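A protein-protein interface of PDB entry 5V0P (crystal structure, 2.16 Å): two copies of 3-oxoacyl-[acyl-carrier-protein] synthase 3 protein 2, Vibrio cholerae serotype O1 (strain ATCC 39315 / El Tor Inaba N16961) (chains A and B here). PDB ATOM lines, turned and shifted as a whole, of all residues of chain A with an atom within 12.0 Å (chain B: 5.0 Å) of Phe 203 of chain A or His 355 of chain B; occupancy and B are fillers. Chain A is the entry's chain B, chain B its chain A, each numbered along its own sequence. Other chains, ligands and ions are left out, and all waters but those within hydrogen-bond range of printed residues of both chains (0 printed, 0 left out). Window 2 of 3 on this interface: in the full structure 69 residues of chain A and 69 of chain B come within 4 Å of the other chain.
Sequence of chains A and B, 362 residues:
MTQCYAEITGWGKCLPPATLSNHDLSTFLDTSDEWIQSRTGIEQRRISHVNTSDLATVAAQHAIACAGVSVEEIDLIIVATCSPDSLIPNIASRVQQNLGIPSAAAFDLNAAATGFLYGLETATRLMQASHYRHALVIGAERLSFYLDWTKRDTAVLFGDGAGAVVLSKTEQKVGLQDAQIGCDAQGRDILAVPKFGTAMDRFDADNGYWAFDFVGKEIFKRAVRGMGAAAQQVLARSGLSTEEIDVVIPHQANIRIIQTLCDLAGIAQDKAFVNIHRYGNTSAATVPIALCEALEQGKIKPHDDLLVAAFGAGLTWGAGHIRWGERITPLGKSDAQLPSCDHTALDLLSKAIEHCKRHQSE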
ATOM      1  N   LYS A 195     -14.084 -21.010 -21.352  1.00  0.00           N
ATOM      2  CA  LYS A 195     -14.265 -21.909 -20.200  1.00  0.00           C
ATOM      3  C   LYS A 195     -13.649 -21.394 -18.892  1.00  0.00           C
ATOM      4  O   LYS A 195     -13.194 -22.177 -18.048  1.00  0.00           O
ATOM      5  CB  LYS A 195     -13.752 -23.323 -20.552  1.00  0.00           C
ATOM      6  CG  LYS A 195     -14.845 -24.265 -21.023  1.00  0.00           C
ATOM      7  CD  LYS A 195     -15.230 -24.005 -22.467  1.00  0.00           C
ATOM      8  CE  LYS A 195     -16.448 -24.850 -22.846  1.00  0.00           C
ATOM      9  NZ  LYS A 195     -17.692 -24.322 -22.209  1.00  0.00           N
ATOM     10  N   PHE A 196     -13.639 -20.075 -18.709  1.00  0.00           N
ATOM     11  CA  PHE A 196     -13.555 -19.537 -17.362  1.00  0.00           C
ATOM     12  C   PHE A 196     -14.746 -18.619 -17.142  1.00  0.00           C
ATOM     13  O   PHE A 196     -14.895 -17.593 -17.824  1.00  0.00           O
ATOM     14  CB  PHE A 196     -12.243 -18.807 -17.052  1.00  0.00           C
ATOM     15  CG  PHE A 196     -12.174 -18.344 -15.624  1.00  0.00           C
ATOM     16  CD1 PHE A 196     -11.825 -19.229 -14.613  1.00  0.00           C
ATOM     17  CD2 PHE A 196     -12.551 -17.050 -15.274  1.00  0.00           C
ATOM     18  CE1 PHE A 196     -11.812 -18.822 -13.291  1.00  0.00           C
ATOM     19  CE2 PHE A 196     -12.544 -16.636 -13.952  1.00  0.00           C
ATOM     20  CZ  PHE A 196     -12.182 -17.520 -12.958  1.00  0.00           C
ATOM     21  N   GLY A 197     -15.552 -18.991 -16.154  1.00  0.00           N
ATOM     22  CA  GLY A 197     -16.832 -18.365 -15.881  1.00  0.00           C
ATOM     23  C   GLY A 197     -17.790 -19.482 -15.552  1.00  0.00           C
ATOM     24  O   GLY A 197     -17.369 -20.604 -15.310  1.00  0.00           O
ATOM     25  N   THR A 198     -19.080 -19.192 -15.584  1.00  0.00           N
ATOM     26  CA  THR A 198     -20.074 -20.175 -15.186  1.00  0.00           C
ATOM     27  C   THR A 198     -20.370 -21.224 -16.272  1.00  0.00           C
ATOM     28  O   THR A 198     -21.117 -22.186 -16.013  1.00  0.00           O
ATOM     29  CB  THR A 198     -21.361 -19.494 -14.698  1.00  0.00           C
ATOM     30  OG1 THR A 198     -22.044 -18.868 -15.796  1.00  0.00           O
ATOM     31  CG2 THR A 198     -21.019 -18.480 -13.611  1.00  0.00           C
ATOM     32  N   ALA A 199     -19.803 -21.024 -17.467  1.00  0.00           N
ATOM     33  CA  ALA A 199     -19.773 -22.051 -18.513  1.00  0.00           C
ATOM     34  C   ALA A 199     -18.808 -23.205 -18.216  1.00  0.00           C
ATOM     35  O   ALA A 199     -18.918 -24.243 -18.855  1.00  0.00           O
ATOM     36  CB  ALA A 199     -19.433 -21.441 -19.871  1.00  0.00           C
ATOM     37  N   MET A 200     -17.874 -23.035 -17.278  1.00  0.00           N
ATOM     38  CA  MET A 200     -16.921 -24.101 -16.937  1.00  0.00           C
ATOM     39  C   MET A 200     -17.571 -25.146 -16.033  1.00  0.00           C
ATOM     40  O   MET A 200     -18.515 -24.844 -15.303  1.00  0.00           O
ATOM     41  CB  MET A 200     -15.662 -23.533 -16.256  1.00  0.00           C
ATOM     42  CG  MET A 200     -15.788 -23.229 -14.767  1.00  0.00           C
ATOM     43  SD  MET A 200     -14.565 -22.031 -14.208  1.00  0.00           S
ATOM     44  CE  MET A 200     -13.063 -22.957 -14.441  1.00  0.00           C
ATOM     45  N   ASP A 201     -17.031 -26.363 -16.080  1.00  0.00           N
ATOM     46  CA  ASP A 201     -17.419 -27.440 -15.171  1.00  0.00           C
ATOM     47  C   ASP A 201     -16.664 -27.240 -13.855  1.00  0.00           C
ATOM     48  O   ASP A 201     -15.453 -27.489 -13.763  1.00  0.00           O
ATOM     49  CB  ASP A 201     -17.099 -28.805 -15.797  1.00  0.00           C
ATOM     50  CG  ASP A 201     -17.629 -29.997 -14.975  1.00  0.00           C
ATOM     51  OD1 ASP A 201     -18.054 -29.846 -13.793  1.00  0.00           O
ATOM     52  OD2 ASP A 201     -17.609 -31.115 -15.541  1.00  0.00           O
ATOM     53  N   ARG A 202     -17.405 -26.796 -12.846  1.00  0.00           N
ATOM     54  CA  ARG A 202     -16.880 -26.511 -11.502  1.00  0.00           C
ATOM     55  C   ARG A 202     -16.143 -27.679 -10.812  1.00  0.00           C
ATOM     56  O   ARG A 202     -15.242 -27.443  -9.997  1.00  0.00           O
ATOM     57  CB  ARG A 202     -18.052 -26.062 -10.612  1.00  0.00           C
ATOM     58  CG  ARG A 202     -17.707 -25.692  -9.180  1.00  0.00           C
ATOM     59  CD  ARG A 202     -18.969 -25.283  -8.451  1.00  0.00           C
ATOM     60  NE  ARG A 202     -18.783 -25.273  -7.007  1.00  0.00           N
ATOM     61  CZ  ARG A 202     -19.753 -25.058  -6.122  1.00  0.00           C
ATOM     62  NH1 ARG A 202     -21.006 -24.793  -6.512  1.00  0.00           N
ATOM     63  NH2 ARG A 202     -19.470 -25.091  -4.827  1.00  0.00           N
ATOM     64  N   PHE A 203     -16.534 -28.917 -11.119  1.00  0.00           N
ATOM     65  CA  PHE A 203     -15.972 -30.094 -10.440  1.00  0.00           C
ATOM     66  C   PHE A 203     -15.042 -30.961 -11.279  1.00  0.00           C
ATOM     67  O   PHE A 203     -14.527 -31.969 -10.782  1.00  0.00           O
ATOM     68  CB  PHE A 203     -17.106 -30.903  -9.805  1.00  0.00           C
ATOM     69  CG  PHE A 203     -17.899 -30.102  -8.822  1.00  0.00           C
ATOM     70  CD1 PHE A 203     -17.344 -29.744  -7.595  1.00  0.00           C
ATOM     71  CD2 PHE A 203     -19.168 -29.626  -9.145  1.00  0.00           C
ATOM     72  CE1 PHE A 203     -18.057 -28.953  -6.695  1.00  0.00           C
ATOM     73  CE2 PHE A 203     -19.885 -28.845  -8.245  1.00  0.00           C
ATOM     74  CZ  PHE A 203     -19.330 -28.510  -7.019  1.00  0.00           C
ATOM     75  N   ASP A 204     -14.793 -30.561 -12.527  1.00  0.00           N
ATOM     76  CA  ASP A 204     -13.776 -31.211 -13.354  1.00  0.00           C
ATOM     77  C   ASP A 204     -12.388 -30.757 -12.896  1.00  0.00           C
ATOM     78  O   ASP A 204     -12.107 -29.546 -12.840  1.00  0.00           O
ATOM     79  CB  ASP A 204     -13.984 -30.867 -14.834  1.00  0.00           C
ATOM     80  CG  ASP A 204     -13.061 -31.650 -15.775  1.00  0.00           C
ATOM     81  OD1 ASP A 204     -12.008 -32.181 -15.335  1.00  0.00           O
ATOM     82  OD2 ASP A 204     -13.389 -31.708 -16.980  1.00  0.00           O
ATOM     83  N   ALA A 205     -11.522 -31.734 -12.607  1.00  0.00           N
ATOM     84  CA  ALA A 205     -10.154 -31.490 -12.144  1.00  0.00           C
ATOM     85  C   ALA A 205      -9.231 -30.948 -13.233  1.00  0.00           C
ATOM     86  O   ALA A 205      -8.185 -30.390 -12.907  1.00  0.00           O
ATOM     87  CB  ALA A 205      -9.550 -32.770 -11.554  1.00  0.00           C
ATOM     88  N   ASP A 206      -9.592 -31.128 -14.508  1.00  0.00           N
ATOM     89  CA  ASP A 206      -8.877 -30.484 -15.628  1.00  0.00           C
ATOM     90  C   ASP A 206      -9.445 -29.105 -16.038  1.00  0.00           C
ATOM     91  O   ASP A 206      -9.006 -28.548 -17.043  1.00  0.00           O
ATOM     92  CB  ASP A 206      -8.868 -31.388 -16.875  1.00  0.00           C
ATOM     93  CG  ASP A 206      -8.145 -32.708 -16.657  1.00  0.00           C
ATOM     94  OD1 ASP A 206      -7.202 -32.780 -15.828  1.00  0.00           O
ATOM     95  OD2 ASP A 206      -8.535 -33.677 -17.345  1.00  0.00           O
ATOM     96  N   ASN A 207     -10.390 -28.546 -15.280  1.00  0.00           N
ATOM     97  CA  ASN A 207     -11.027 -27.268 -15.673  1.00  0.00           C
ATOM     98  C   ASN A 207     -10.071 -26.051 -15.757  1.00  0.00           C
ATOM     99  O   ASN A 207     -10.398 -25.046 -16.397  1.00  0.00           O
ATOM    100  CB  ASN A 207     -12.278 -26.966 -14.806  1.00  0.00           C
ATOM    101  CG  ASN A 207     -11.949 -26.601 -13.360  1.00  0.00           C
ATOM    102  OD1 ASN A 207     -10.787 -26.420 -12.987  1.00  0.00           O
ATOM    103  ND2 ASN A 207     -12.987 -26.509 -12.532  1.00  0.00           N
ATOM    104  N   GLY A 208      -8.912 -26.146 -15.101  1.00  0.00           N
ATOM    105  CA  GLY A 208      -7.866 -25.122 -15.173  1.00  0.00           C
ATOM    106  C   GLY A 208      -7.082 -25.004 -16.478  1.00  0.00           C
ATOM    107  O   GLY A 208      -6.370 -24.010 -16.683  1.00  0.00           O
ATOM    108  N   TYR A 209      -7.186 -26.005 -17.357  1.00  0.00           N
ATOM    109  CA  TYR A 209      -6.410 -26.051 -18.600  1.00  0.00           C
ATOM    110  C   TYR A 209      -7.301 -25.620 -19.758  1.00  0.00           C
ATOM    111  O   TYR A 209      -7.570 -26.392 -20.680  1.00  0.00           O
ATOM    112  CB  TYR A 209      -5.814 -27.464 -18.793  1.00  0.00           C
ATOM    113  CG  TYR A 209      -4.997 -27.902 -17.593  1.00  0.00           C
ATOM    114  CD1 TYR A 209      -3.731 -27.361 -17.356  1.00  0.00           C
ATOM    115  CD2 TYR A 209      -5.508 -28.811 -16.661  1.00  0.00           C
ATOM    116  CE1 TYR A 209      -2.981 -27.733 -16.245  1.00  0.00           C
ATOM    117  CE2 TYR A 209      -4.765 -29.194 -15.541  1.00  0.00           C
ATOM    118  CZ  TYR A 209      -3.502 -28.650 -15.337  1.00  0.00           C
ATOM    119  OH  TYR A 209      -2.746 -29.008 -14.237  1.00  0.00           O
ATOM    120  N   TRP A 210      -7.745 -24.360 -19.696  1.00  0.00           N
ATOM    121  CA  TRP A 210      -8.653 -23.794 -20.696  1.00  0.00           C
ATOM    122  C   TRP A 210      -7.914 -23.302 -21.928  1.00  0.00           C
ATOM    123  O   TRP A 210      -6.748 -22.911 -21.856  1.00  0.00           O
ATOM    124  CB  TRP A 210      -9.521 -22.663 -20.107  1.00  0.00           C
ATOM    125  CG  TRP A 210      -8.785 -21.592 -19.382  1.00  0.00           C
ATOM    126  CD1 TRP A 210      -7.927 -20.676 -19.912  1.00  0.00           C
ATOM    127  CD2 TRP A 210      -8.850 -21.321 -17.980  1.00  0.00           C
ATOM    128  NE1 TRP A 210      -7.451 -19.854 -18.923  1.00  0.00           N
ATOM    129  CE2 TRP A 210      -7.999 -20.230 -17.727  1.00  0.00           C
ATOM    130  CE3 TRP A 210      -9.541 -21.900 -16.911  1.00  0.00           C
ATOM    131  CZ2 TRP A 210      -7.830 -19.694 -16.441  1.00  0.00           C
ATOM    132  CZ3 TRP A 210      -9.372 -21.374 -15.635  1.00  0.00           C
ATOM    133  CH2 TRP A 210      -8.534 -20.277 -15.411  1.00  0.00           C
ATOM    134  N   GLY B 208     -13.031 -26.007  -6.583  1.00  0.00           N
ATOM    135  CA  GLY B 208     -14.489 -26.027  -6.726  1.00  0.00           C
ATOM    136  C   GLY B 208     -15.328 -26.028  -5.449  1.00  0.00           C
ATOM    137  O   GLY B 208     -16.542 -25.779  -5.508  1.00  0.00           O
ATOM    138  N   TYR B 209     -14.705 -26.298  -4.298  1.00  0.00           N
ATOM    139  CA  TYR B 209     -15.416 -26.403  -3.019  1.00  0.00           C
ATOM    140  C   TYR B 209     -15.222 -25.109  -2.236  1.00  0.00           C
ATOM    141  O   TYR B 209     -14.632 -25.090  -1.159  1.00  0.00           O
ATOM    142  CB  TYR B 209     -14.926 -27.651  -2.247  1.00  0.00           C
ATOM    143  CG  TYR B 209     -15.051 -28.915  -3.083  1.00  0.00           C
ATOM    144  CD1 TYR B 209     -16.295 -29.499  -3.301  1.00  0.00           C
ATOM    145  CD2 TYR B 209     -13.938 -29.489  -3.707  1.00  0.00           C
ATOM    146  CE1 TYR B 209     -16.432 -30.638  -4.084  1.00  0.00           C
ATOM    147  CE2 TYR B 209     -14.062 -30.628  -4.499  1.00  0.00           C
ATOM    148  CZ  TYR B 209     -15.314 -31.205  -4.683  1.00  0.00           C
ATOM    149  OH  TYR B 209     -15.466 -32.335  -5.466  1.00  0.00           O
ATOM    150  N   SER B 350     -27.526 -33.167  -9.759  1.00  0.00           N
ATOM    151  CA  SER B 350     -26.968 -34.455  -9.255  1.00  0.00           C
ATOM    152  C   SER B 350     -25.434 -34.468  -9.159  1.00  0.00           C
ATOM    153  O   SER B 350     -24.889 -34.648  -8.072  1.00  0.00           O
ATOM    154  CB  SER B 350     -27.473 -35.644 -10.095  1.00  0.00           C
ATOM    155  OG  SER B 350     -27.149 -35.482 -11.467  1.00  0.00           O
ATOM    156  N   LYS B 351     -24.749 -34.238 -10.280  1.00  0.00           N
ATOM    157  CA  LYS B 351     -23.280 -34.124 -10.294  1.00  0.00           C
ATOM    158  C   LYS B 351     -22.735 -33.152  -9.228  1.00  0.00           C
ATOM    159  O   LYS B 351     -21.776 -33.485  -8.513  1.00  0.00           O
ATOM    160  CB  LYS B 351     -22.779 -33.698 -11.682  1.00  0.00           C
ATOM    161  N   ALA B 352     -23.359 -31.977  -9.112  1.00  0.00           N
ATOM    162  CA  ALA B 352     -22.934 -30.949  -8.147  1.00  0.00           C
ATOM    163  C   ALA B 352     -23.213 -31.359  -6.697  1.00  0.00           C
ATOM    164  O   ALA B 352     -22.353 -31.207  -5.833  1.00  0.00           O
ATOM    165  CB  ALA B 352     -23.593 -29.597  -8.460  1.00  0.00           C
ATOM    166  N   ILE B 353     -24.414 -31.869  -6.441  1.00  0.00           N
ATOM    167  CA  ILE B 353     -24.793 -32.342  -5.103  1.00  0.00           C
ATOM    168  C   ILE B 353     -23.884 -33.495  -4.653  1.00  0.00           C
ATOM    169  O   ILE B 353     -23.426 -33.502  -3.505  1.00  0.00           O
ATOM    170  CB  ILE B 353     -26.283 -32.781  -5.041  1.00  0.00           C
ATOM    171  CG1 ILE B 353     -27.206 -31.565  -5.183  1.00  0.00           C
ATOM    172  CG2 ILE B 353     -26.602 -33.512  -3.733  1.00  0.00           C
ATOM    173  CD1 ILE B 353     -28.646 -31.899  -5.514  1.00  0.00           C
ATOM    174  N   GLU B 354     -23.634 -34.457  -5.550  1.00  0.00           N
ATOM    175  CA  GLU B 354     -22.831 -35.658  -5.219  1.00  0.00           C
ATOM    176  C   GLU B 354     -21.361 -35.319  -4.909  1.00  0.00           C
ATOM    177  O   GLU B 354     -20.768 -35.915  -4.003  1.00  0.00           O
ATOM    178  CB  GLU B 354     -22.909 -36.709  -6.342  1.00  0.00           C
ATOM    179  N   HIS B 355     -20.790 -34.368  -5.654  1.00  0.00           N
ATOM    180  CA  HIS B 355     -19.422 -33.888  -5.393  1.00  0.00           C
ATOM    181  C   HIS B 355     -19.320 -33.122  -4.072  1.00  0.00           C
ATOM    182  O   HIS B 355     -18.367 -33.319  -3.315  1.00  0.00           O
ATOM    183  CB  HIS B 355     -18.904 -33.012  -6.542  1.00  0.00           C
ATOM    184  CG  HIS B 355     -18.399 -33.785  -7.723  1.00  0.00           C
ATOM    185  ND1 HIS B 355     -19.151 -33.989  -8.863  1.00  0.00           N
ATOM    186  CD2 HIS B 355     -17.202 -34.374  -7.954  1.00  0.00           C
ATOM    187  CE1 HIS B 355     -18.448 -34.688  -9.735  1.00  0.00           C
ATOM    188  NE2 HIS B 355     -17.260 -34.931  -9.211  1.00  0.00           N
ATOM    189  N   CYS B 356     -20.286 -32.245  -3.805  1.00  0.00           N
ATOM    190  CA  CYS B 356     -20.306 -31.474  -2.554  1.00  0.00           C
ATOM    191  C   CYS B 356     -20.432 -32.387  -1.329  1.00  0.00           C
ATOM    192  O   CYS B 356     -19.718 -32.200  -0.341  1.00  0.00           O
ATOM    193  CB  CYS B 356     -21.437 -30.443  -2.554  1.00  0.00           C
ATOM    194  SG  CYS B 356     -21.152 -29.037  -3.652  1.00  0.00           S
ATOM    195  N   LYS B 357     -21.338 -33.363  -1.407  1.00  0.00           N
ATOM    196  CA  LYS B 357     -21.550 -34.317  -0.311  1.00  0.00           C
ATOM    197  C   LYS B 357     -20.377 -35.289  -0.127  1.00  0.00           C
ATOM    198  O   LYS B 357     -20.072 -35.669   1.003  1.00  0.00           O
ATOM    199  CB  LYS B 357     -22.879 -35.067  -0.480  1.00  0.00           C
ATOM    200  CG  LYS B 357     -24.056 -34.309   0.134  1.00  0.00           C
ATOM    201  CD  LYS B 357     -25.402 -34.699  -0.456  1.00  0.00           C
ATOM    202  CE  LYS B 357     -25.847 -36.077  -0.004  1.00  0.00           C
ATOM    203  NZ  LYS B 357     -27.119 -36.494  -0.660  1.00  0.00           N
ATOM    204  N   ARG B 358     -19.724 -35.678  -1.225  1.00  0.00           N
ATOM    205  CA  ARG B 358     -18.534 -36.547  -1.161  1.00  0.00           C
ATOM    206  C   ARG B 358     -17.304 -35.829  -0.583  1.00  0.00           C
ATOM    207  O   ARG B 358     -16.527 -36.438   0.154  1.00  0.00           O
ATOM    208  CB  ARG B 358     -18.202 -37.130  -2.541  1.00  0.00           C
ATOM    209  N   HIS B 359     -17.130 -34.549  -0.918  1.00  0.00           N
ATOM    210  CA  HIS B 359     -16.021 -33.732  -0.388  1.00  0.00           C
ATOM    211  C   HIS B 359     -16.115 -33.465   1.127  1.00  0.00           C
ATOM    212  O   HIS B 359     -15.086 -33.406   1.811  1.00  0.00           O
ATOM    213  CB  HIS B 359     -15.925 -32.400  -1.154  1.00  0.00           C
ATOM    214  CG  HIS B 359     -14.805 -31.512  -0.700  1.00  0.00           C
ATOM    215  ND1 HIS B 359     -14.985 -30.491   0.212  1.00  0.00           N
ATOM    216  CD2 HIS B 359     -13.490 -31.499  -1.025  1.00  0.00           C
ATOM    217  CE1 HIS B 359     -13.830 -29.885   0.424  1.00  0.00           C
ATOM    218  NE2 HIS B 359     -12.908 -30.476  -0.316  1.00  0.00           N
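The guanidinium group (NE) of Arg 202 of chain A lies within hydrogen-bond range of the backbone carbonyl oxygen (O) of Gly 208 of chain B.
Of chain B, only Gly 208 (3.7 Å), Tyr 209 (3.5 Å), Ala 352 (3.7 Å), His 355 (3.8 Å) and Cys 356 (3.9 Å) come within 4 Å of Phe 203 of chain A.
His 355 of chain B touches one residue of chain A.
Gly 208 of chain B touches two residues of chain A.
Of chain A, only Phe 203 (3.5 Å) comes within 4 Å of Tyr 209 of chain B.
Of chain A, only Phe 203 (3.9 Å) comes within 4 Å of Cys 356 of chain B.
No residue of chain A comes within 4 Å of His 359 of chain B.
Of the printed residues of chain B, Arg 202 of chain A touches Gly 208.
Ser 350 of chain B touches none of the printed residues of chain A.
Of the 16 printed residues of chain A, 2 touch a printed residue of chain B.
Hydrophobic or aromatic side chains of chain A that line the printed part of chain B: Phe 203.
Of the 12 printed residues of chain B, 5 touch a printed residue of chain A.
Phe 203 of chain A touches Gly 208 of chain B (CE1 to O, 3.7 Å).
Tyr 209 of chain B touches Phe 203 of chain A (CE1 to CE1, 3.5 Å).
CE2 of Phe 203 of chain A touches CA of Ala 352 of chain B, at 3.7 Å.
CD1 of Phe 203 of chain A touches CB of His 355 of chain B (3.8 Å).
Phe 203 of chain A touches Cys 356 of chain B.
O of Lys 351 of chain B lies within hydrogen-bond range of ND1 of His 355 of chain B (2.7 Å).
O of Ala 352 of chain B sits at hydrogen-bond distance from SG of Cys 356 of chain B.
The backbone NH (N) of Phe 203 of chain A lies close to the side-chain carboxylate (OD1) of Asp 201 of chain A, at 3.2 Å.
Positions printed for both chains: 208 and 209.
Of the 6 pairs that touch across the chains among the printed residues, none has its exchanged pair printed and touching as well.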
